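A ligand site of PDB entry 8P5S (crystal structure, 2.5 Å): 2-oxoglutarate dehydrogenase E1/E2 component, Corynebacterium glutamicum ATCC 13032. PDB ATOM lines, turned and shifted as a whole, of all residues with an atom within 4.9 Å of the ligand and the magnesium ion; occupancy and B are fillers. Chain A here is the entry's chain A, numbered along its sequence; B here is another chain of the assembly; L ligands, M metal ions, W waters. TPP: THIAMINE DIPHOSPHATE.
The magnesium ion is bound by O2A of the ligand (2.0 Å), O3B of the ligand (2.1 Å), OD1 of Asn 582 (2.2 Å), O of Ile 584 (2.2 Å), OD1 of Asp 549 (2.2 Å) and water W2 (2.5 Å).
The side-chain amide oxygen (OE1) of Gln 877 of chain B sits close to a nitrogen (N3) of the ligand.
Residues that only touch the ligand: His 513 (3.5 Å), Gly 548 (3.4 Å), Gly 585 (3.5 Å), Glu 805 of chain B (3.2 Å), Leu 851 of chain B (3.5 Å) and Phe 881 of chain B (3.3 Å).
An oxygen (O2A) of the ligand sits close to the backbone NH of Asp 549 (3.5 Å).
The backbone NH (N) of Ala 551 lies within hydrogen-bond range of an oxygen (O1A) of the ligand (2.9 Å).
N of Ala 550 lies within hydrogen-bond range of O1A of the ligand, 3.4 Å away.
OE2 of Glu 853 of chain B lies within hydrogen-bond range of N1' of the ligand (2.8 Å).
The backbone NH (N) of Leu 514 lies within hydrogen-bond range of a nitrogen (N3') of the ligand (3.0 Å).
A ring nitrogen (NE2) of His 651 sits close to a sulfur (S1) of the ligand (3.6 Å).
NE of Arg 448 lies within salt-bridge range of O1B of the ligand (3.0 Å).
O of Ser 512 is in hydrogen-bond range of N4' of the ligand (2.9 Å).
Of the 23 residues printed, 3 come within 4 Å of the magnesium ion.
Water W2 lies within hydrogen-bond range of O of Val 580 (2.4 Å), O1B of the ligand (2.8 Å) and ND2 of Asn 582 (3.3 Å).
Water W1 lies within hydrogen-bond range of ND1 of His 651 (2.7 Å), N of Phe 586 (2.9 Å) and O2B of the ligand (3.0 Å).
NE2 of Gln 877 of chain B sits at hydrogen-bond distance from OD2 of Asp 806 of chain B, at 2.9 Å.
NE2 of Gln 877 of chain B sits at hydrogen-bond distance from O of Glu 805 of chain B, 3.3 Å away.
O of Leu 851 of chain B lies within hydrogen-bond range of N of Leu 555.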
ATOM      1  N   HIS A 447       2.191  12.758  12.963  1.00  0.00           N
ATOM      2  CA  HIS A 447       2.235  13.027  14.396  1.00  0.00           C
ATOM      3  C   HIS A 447       2.370  14.502  14.776  1.00  0.00           C
ATOM      4  O   HIS A 447       1.785  14.899  15.775  1.00  0.00           O
ATOM      5  CB  HIS A 447       3.373  12.220  15.051  1.00  0.00           C
ATOM      6  CG  HIS A 447       4.724  12.431  14.432  1.00  0.00           C
ATOM      7  ND1 HIS A 447       5.046  11.894  13.200  1.00  0.00           N
ATOM      8  CD2 HIS A 447       5.804  13.103  14.918  1.00  0.00           C
ATOM      9  CE1 HIS A 447       6.290  12.285  12.951  1.00  0.00           C
ATOM     10  NE2 HIS A 447       6.787  13.012  13.952  1.00  0.00           N
ATOM     11  N   ARG A 448       3.164  15.298  14.069  1.00  0.00           N
ATOM     12  CA  ARG A 448       3.415  16.696  14.454  1.00  0.00           C
ATOM     13  C   ARG A 448       2.150  17.532  14.633  1.00  0.00           C
ATOM     14  O   ARG A 448       1.443  17.801  13.672  1.00  0.00           O
ATOM     15  CB  ARG A 448       4.325  17.393  13.419  1.00  0.00           C
ATOM     16  CG  ARG A 448       4.752  18.812  13.814  1.00  0.00           C
ATOM     17  CD  ARG A 448       5.957  19.357  13.057  1.00  0.00           C
ATOM     18  NE  ARG A 448       7.082  18.416  12.962  1.00  0.00           N
ATOM     19  CZ  ARG A 448       8.048  18.298  13.862  1.00  0.00           C
ATOM     20  NH1 ARG A 448       9.014  17.417  13.695  1.00  0.00           N
ATOM     21  NH2 ARG A 448       8.059  19.060  14.948  1.00  0.00           N
ATOM     22  N   SER A 512       3.220   4.828  11.601  1.00  0.00           N
ATOM     23  CA  SER A 512       4.318   5.797  11.602  1.00  0.00           C
ATOM     24  C   SER A 512       4.931   5.965  10.210  1.00  0.00           C
ATOM     25  O   SER A 512       5.565   6.987   9.965  1.00  0.00           O
ATOM     26  CB  SER A 512       5.393   5.425  12.604  1.00  0.00           C
ATOM     27  OG  SER A 512       4.834   5.362  13.907  1.00  0.00           O
ATOM     28  N   HIS A 513       4.724   5.011   9.287  1.00  0.00           N
ATOM     29  CA  HIS A 513       5.157   5.135   7.887  1.00  0.00           C
ATOM     30  C   HIS A 513       4.466   6.355   7.287  1.00  0.00           C
ATOM     31  O   HIS A 513       3.246   6.386   7.193  1.00  0.00           O
ATOM     32  CB  HIS A 513       4.776   3.859   7.095  1.00  0.00           C
ATOM     33  CG  HIS A 513       5.486   2.612   7.517  1.00  0.00           C
ATOM     34  ND1 HIS A 513       5.476   2.191   8.845  1.00  0.00           N
ATOM     35  CD2 HIS A 513       6.171   1.715   6.779  1.00  0.00           C
ATOM     36  CE1 HIS A 513       6.166   1.057   8.868  1.00  0.00           C
ATOM     37  NE2 HIS A 513       6.619   0.746   7.651  1.00  0.00           N
ATOM     38  N   LEU A 514       5.239   7.405   7.048  1.00  0.00           N
ATOM     39  CA  LEU A 514       4.692   8.653   6.561  1.00  0.00           C
ATOM     40  C   LEU A 514       4.011   8.495   5.208  1.00  0.00           C
ATOM     41  O   LEU A 514       4.401   7.643   4.394  1.00  0.00           O
ATOM     42  CB  LEU A 514       5.814   9.692   6.474  1.00  0.00           C
ATOM     43  CG  LEU A 514       6.450  10.111   7.810  1.00  0.00           C
ATOM     44  CD1 LEU A 514       7.705  10.969   7.599  1.00  0.00           C
ATOM     45  CD2 LEU A 514       5.431  10.818   8.717  1.00  0.00           C
ATOM     46  N   GLY A 548       4.343  16.632   5.628  1.00  0.00           N
ATOM     47  CA  GLY A 548       5.607  17.280   5.953  1.00  0.00           C
ATOM     48  C   GLY A 548       6.333  17.526   4.623  1.00  0.00           C
ATOM     49  O   GLY A 548       6.107  16.799   3.659  1.00  0.00           O
ATOM     50  N   ASP A 549       7.189  18.541   4.538  1.00  0.00           N
ATOM     51  CA  ASP A 549       7.869  18.895   3.287  1.00  0.00           C
ATOM     52  C   ASP A 549       8.819  17.820   2.766  1.00  0.00           C
ATOM     53  O   ASP A 549       8.934  17.684   1.550  1.00  0.00           O
ATOM     54  CB  ASP A 549       8.633  20.208   3.431  1.00  0.00           C
ATOM     55  CG  ASP A 549       9.569  20.226   4.628  1.00  0.00           C
ATOM     56  OD1 ASP A 549       9.065  20.251   5.769  1.00  0.00           O
ATOM     57  OD2 ASP A 549      10.805  20.234   4.412  1.00  0.00           O
ATOM     58  N   ALA A 550       9.522  17.128   3.642  1.00  0.00           N
ATOM     59  CA  ALA A 550      10.471  16.108   3.200  1.00  0.00           C
ATOM     60  C   ALA A 550       9.726  14.874   2.675  1.00  0.00           C
ATOM     61  O   ALA A 550      10.077  14.341   1.612  1.00  0.00           O
ATOM     62  CB  ALA A 550      11.391  15.728   4.362  1.00  0.00           C
ATOM     63  N   ALA A 551       8.665  14.464   3.383  1.00  0.00           N
ATOM     64  CA  ALA A 551       7.865  13.302   3.019  1.00  0.00           C
ATOM     65  C   ALA A 551       7.000  13.533   1.784  1.00  0.00           C
ATOM     66  O   ALA A 551       6.817  12.607   0.993  1.00  0.00           O
ATOM     67  CB  ALA A 551       6.982  12.905   4.183  1.00  0.00           C
ATOM     68  N   LEU A 555       8.343  10.650  -0.997  1.00  0.00           N
ATOM     69  CA  LEU A 555       7.644   9.372  -1.087  1.00  0.00           C
ATOM     70  C   LEU A 555       6.721   9.357  -2.282  1.00  0.00           C
ATOM     71  O   LEU A 555       5.939  10.283  -2.442  1.00  0.00           O
ATOM     72  CB  LEU A 555       6.883   9.097   0.217  1.00  0.00           C
ATOM     73  CG  LEU A 555       7.785   8.823   1.410  1.00  0.00           C
ATOM     74  CD1 LEU A 555       7.027   8.934   2.709  1.00  0.00           C
ATOM     75  CD2 LEU A 555       8.472   7.475   1.290  1.00  0.00           C
ATOM     76  N   VAL A 580       3.171  21.376   5.795  1.00  0.00           N
ATOM     77  CA  VAL A 580       3.851  22.092   6.849  1.00  0.00           C
ATOM     78  C   VAL A 580       5.334  22.075   6.481  1.00  0.00           C
ATOM     79  O   VAL A 580       6.064  21.138   6.797  1.00  0.00           O
ATOM     80  CB  VAL A 580       3.559  21.454   8.226  1.00  0.00           C
ATOM     81  CG1 VAL A 580       4.268  22.194   9.341  1.00  0.00           C
ATOM     82  CG2 VAL A 580       2.063  21.407   8.477  1.00  0.00           C
ATOM     83  N   ASN A 582       8.556  23.132   7.059  1.00  0.00           N
ATOM     84  CA  ASN A 582       9.451  23.727   8.044  1.00  0.00           C
ATOM     85  C   ASN A 582      10.925  23.703   7.603  1.00  0.00           C
ATOM     86  O   ASN A 582      11.808  23.870   8.431  1.00  0.00           O
ATOM     87  CB  ASN A 582       9.280  23.072   9.411  1.00  0.00           C
ATOM     88  CG  ASN A 582       9.397  21.573   9.427  1.00  0.00           C
ATOM     89  OD1 ASN A 582       9.916  20.948   8.504  1.00  0.00           O
ATOM     90  ND2 ASN A 582       8.903  20.972  10.486  1.00  0.00           N
ATOM     91  N   GLN A 583      11.170  23.495   6.295  1.00  0.00           N
ATOM     92  CA  GLN A 583      12.445  23.556   5.603  1.00  0.00           C
ATOM     93  C   GLN A 583      13.503  22.635   6.208  1.00  0.00           C
ATOM     94  O   GLN A 583      14.692  22.938   6.121  1.00  0.00           O
ATOM     95  CB  GLN A 583      12.933  25.018   5.583  1.00  0.00           C
ATOM     96  CG  GLN A 583      11.834  25.993   5.169  1.00  0.00           C
ATOM     97  CD  GLN A 583      12.287  27.413   5.226  1.00  0.00           C
ATOM     98  OE1 GLN A 583      13.251  27.794   4.566  1.00  0.00           O
ATOM     99  NE2 GLN A 583      11.605  28.228   6.000  1.00  0.00           N
ATOM    100  N   ILE A 584      13.080  21.517   6.786  1.00  0.00           N
ATOM    101  CA  ILE A 584      13.940  20.500   7.373  1.00  0.00           C
ATOM    102  C   ILE A 584      13.164  19.161   7.500  1.00  0.00           C
ATOM    103  O   ILE A 584      11.926  19.135   7.537  1.00  0.00           O
ATOM    104  CB  ILE A 584      14.492  20.996   8.738  1.00  0.00           C
ATOM    105  CG1 ILE A 584      15.697  20.158   9.198  1.00  0.00           C
ATOM    106  CG2 ILE A 584      13.411  21.075   9.782  1.00  0.00           C
ATOM    107  CD1 ILE A 584      16.477  20.774  10.241  1.00  0.00           C
ATOM    108  N   GLY A 585      13.907  18.064   7.518  1.00  0.00           N
ATOM    109  CA  GLY A 585      13.395  16.709   7.697  1.00  0.00           C
ATOM    110  C   GLY A 585      14.413  15.936   8.518  1.00  0.00           C
ATOM    111  O   GLY A 585      15.362  15.394   7.948  1.00  0.00           O
ATOM    112  N   PHE A 586      14.236  15.903   9.854  1.00  0.00           N
ATOM    113  CA  PHE A 586      15.127  15.306  10.852  1.00  0.00           C
ATOM    114  C   PHE A 586      16.476  16.101  10.804  1.00  0.00           C
ATOM    115  O   PHE A 586      16.522  17.186  11.364  1.00  0.00           O
ATOM    116  CB  PHE A 586      15.264  13.763  10.700  1.00  0.00           C
ATOM    117  CG  PHE A 586      15.780  13.033  11.916  1.00  0.00           C
ATOM    118  CD1 PHE A 586      16.511  13.692  12.899  1.00  0.00           C
ATOM    119  CD2 PHE A 586      15.555  11.675  12.081  1.00  0.00           C
ATOM    120  CE1 PHE A 586      16.956  13.024  14.031  1.00  0.00           C
ATOM    121  CE2 PHE A 586      16.040  10.995  13.206  1.00  0.00           C
ATOM    122  CZ  PHE A 586      16.733  11.677  14.175  1.00  0.00           C
ATOM    123  N   HIS A 651      14.477  17.342  16.200  1.00  0.00           N
ATOM    124  CA  HIS A 651      13.559  16.284  15.776  1.00  0.00           C
ATOM    125  C   HIS A 651      13.127  15.398  16.950  1.00  0.00           C
ATOM    126  O   HIS A 651      11.990  14.919  16.955  1.00  0.00           O
ATOM    127  CB  HIS A 651      14.165  15.439  14.663  1.00  0.00           C
ATOM    128  CG  HIS A 651      13.230  14.426  14.073  1.00  0.00           C
ATOM    129  ND1 HIS A 651      12.251  14.787  13.159  1.00  0.00           N
ATOM    130  CD2 HIS A 651      13.145  13.095  14.285  1.00  0.00           C
ATOM    131  CE1 HIS A 651      11.619  13.666  12.842  1.00  0.00           C
ATOM    132  NE2 HIS A 651      12.123  12.619  13.499  1.00  0.00           N
ATOM    133  N   GLU B 805      18.551   7.701   5.183  1.00  0.00           N
ATOM    134  CA  GLU B 805      17.978   8.875   5.823  1.00  0.00           C
ATOM    135  C   GLU B 805      18.774   9.275   7.055  1.00  0.00           C
ATOM    136  O   GLU B 805      18.896   8.472   7.994  1.00  0.00           O
ATOM    137  CB  GLU B 805      16.515   8.629   6.186  1.00  0.00           C
ATOM    138  CG  GLU B 805      15.623   8.547   4.968  1.00  0.00           C
ATOM    139  CD  GLU B 805      14.310   7.817   5.172  1.00  0.00           C
ATOM    140  OE1 GLU B 805      13.978   7.485   6.321  1.00  0.00           O
ATOM    141  OE2 GLU B 805      13.619   7.567   4.158  1.00  0.00           O
ATOM    142  N   ASP B 806      19.341  10.496   7.041  1.00  0.00           N
ATOM    143  CA  ASP B 806      20.096  11.117   8.140  1.00  0.00           C
ATOM    144  C   ASP B 806      21.316  10.277   8.508  1.00  0.00           C
ATOM    145  O   ASP B 806      21.653  10.140   9.671  1.00  0.00           O
ATOM    146  CB  ASP B 806      19.178  11.297   9.363  1.00  0.00           C
ATOM    147  CG  ASP B 806      17.899  12.012   9.004  1.00  0.00           C
ATOM    148  OD1 ASP B 806      17.950  13.248   8.833  1.00  0.00           O
ATOM    149  OD2 ASP B 806      16.845  11.326   8.867  1.00  0.00           O
ATOM    150  N   LEU B 851      13.630  11.293   1.473  1.00  0.00           N
ATOM    151  CA  LEU B 851      12.705  10.484   2.243  1.00  0.00           C
ATOM    152  C   LEU B 851      12.085   9.472   1.284  1.00  0.00           C
ATOM    153  O   LEU B 851      11.022   9.725   0.690  1.00  0.00           O
ATOM    154  CB  LEU B 851      11.650  11.429   2.837  1.00  0.00           C
ATOM    155  CG  LEU B 851      10.801  11.032   4.058  1.00  0.00           C
ATOM    156  CD1 LEU B 851      10.941   9.582   4.496  1.00  0.00           C
ATOM    157  CD2 LEU B 851      10.932  12.048   5.150  1.00  0.00           C
ATOM    158  N   GLU B 853      12.228   4.863   0.405  1.00  0.00           N
ATOM    159  CA  GLU B 853      12.738   3.530   0.681  1.00  0.00           C
ATOM    160  C   GLU B 853      12.825   2.726  -0.603  1.00  0.00           C
ATOM    161  O   GLU B 853      13.826   2.082  -0.844  1.00  0.00           O
ATOM    162  CB  GLU B 853      11.883   2.786   1.706  1.00  0.00           C
ATOM    163  CG  GLU B 853      12.209   3.197   3.121  1.00  0.00           C
ATOM    164  CD  GLU B 853      11.400   4.395   3.573  1.00  0.00           C
ATOM    165  OE1 GLU B 853      10.249   4.540   3.111  1.00  0.00           O
ATOM    166  OE2 GLU B 853      11.916   5.179   4.403  1.00  0.00           O
ATOM    167  N   GLN B 877      15.989   4.216   8.326  1.00  0.00           N
ATOM    168  CA  GLN B 877      15.833   5.000   9.563  1.00  0.00           C
ATOM    169  C   GLN B 877      15.556   4.032  10.730  1.00  0.00           C
ATOM    170  O   GLN B 877      16.273   4.005  11.714  1.00  0.00           O
ATOM    171  CB  GLN B 877      14.760   6.075   9.414  1.00  0.00           C
ATOM    172  CG  GLN B 877      14.627   6.945  10.636  1.00  0.00           C
ATOM    173  CD  GLN B 877      14.918   8.391  10.328  1.00  0.00           C
ATOM    174  OE1 GLN B 877      14.065   9.248  10.496  1.00  0.00           O
ATOM    175  NE2 GLN B 877      16.130   8.665   9.869  1.00  0.00           N
ATOM    176  N   PHE B 881      10.513   0.391   8.269  1.00  0.00           N
ATOM    177  CA  PHE B 881      10.134   1.146   7.076  1.00  0.00           C
ATOM    178  C   PHE B 881      10.630   0.509   5.777  1.00  0.00           C
ATOM    179  O   PHE B 881      10.284   1.009   4.717  1.00  0.00           O
ATOM    180  CB  PHE B 881      10.644   2.596   7.157  1.00  0.00           C
ATOM    181  CG  PHE B 881      10.060   3.300   8.341  1.00  0.00           C
ATOM    182  CD1 PHE B 881       8.694   3.291   8.557  1.00  0.00           C
ATOM    183  CD2 PHE B 881      10.869   3.944   9.262  1.00  0.00           C
ATOM    184  CE1 PHE B 881       8.142   3.931   9.660  1.00  0.00           C
ATOM    185  CE2 PHE B 881      10.318   4.575  10.370  1.00  0.00           C
ATOM    186  CZ  PHE B 881       8.965   4.549  10.573  1.00  0.00           C
HETATM  187  N1' TPP L   1      10.093   6.549   6.098  1.00  0.00           N
HETATM  188  C2' TPP L   1       8.775   6.477   6.359  1.00  0.00           C
HETATM  189  CM2 TPP L   1       7.904   5.905   5.286  1.00  0.00           C
HETATM  190  N3' TPP L   1       8.183   6.867   7.491  1.00  0.00           N
HETATM  191  C4' TPP L   1       8.959   7.367   8.470  1.00  0.00           C
HETATM  192  N4' TPP L   1       8.348   7.693   9.614  1.00  0.00           N
HETATM  193  C5' TPP L   1      10.368   7.497   8.301  1.00  0.00           C
HETATM  194  C6' TPP L   1      10.850   7.062   7.082  1.00  0.00           C
HETATM  195  C7' TPP L   1      11.284   8.081   9.346  1.00  0.00           C
HETATM  196  N3  TPP L   1      11.005   9.508   9.644  1.00  0.00           N
HETATM  197  C2  TPP L   1      10.263   9.919  10.653  1.00  0.00           C
HETATM  198  S1  TPP L   1      10.105  11.587  10.702  1.00  0.00           S
HETATM  199  C5  TPP L   1      11.076  11.766   9.291  1.00  0.00           C
HETATM  200  C4  TPP L   1      11.499  10.551   8.854  1.00  0.00           C
HETATM  201  CM4 TPP L   1      12.453  10.288   7.724  1.00  0.00           C
HETATM  202  C6  TPP L   1      11.312  13.115   8.667  1.00  0.00           C
HETATM  203  C7  TPP L   1      10.026  13.843   8.333  1.00  0.00           C
HETATM  204  O7  TPP L   1      10.355  15.024   7.550  1.00  0.00           O
HETATM  205  PA  TPP L   1       9.179  16.000   7.067  1.00  0.00           P
HETATM  206  O1A TPP L   1       8.297  15.208   6.179  1.00  0.00           O
HETATM  207  O2A TPP L   1       9.723  17.295   6.583  1.00  0.00           O
HETATM  208  O3A TPP L   1       8.417  16.217   8.457  1.00  0.00           O
HETATM  209  PB  TPP L   1       8.676  17.114   9.791  1.00  0.00           P
HETATM  210  O1B TPP L   1       7.300  17.694  10.083  1.00  0.00           O
HETATM  211  O2B TPP L   1       9.172  16.201  10.884  1.00  0.00           O
HETATM  212  O3B TPP L   1       9.689  18.160   9.379  1.00  0.00           O
HETATM  213 MG    MG M   1       9.758  19.055   7.485  1.00  0.00          MG
HETATM  214  O   HOH W   1      12.029  16.941  11.467  1.00  0.00           O
HETATM  215  O   HOH W   2       7.363  19.505   8.006  1.00  0.00           O
HETATM  216  O   HOH W   3       9.409   7.468  12.360  1.00  0.00           O
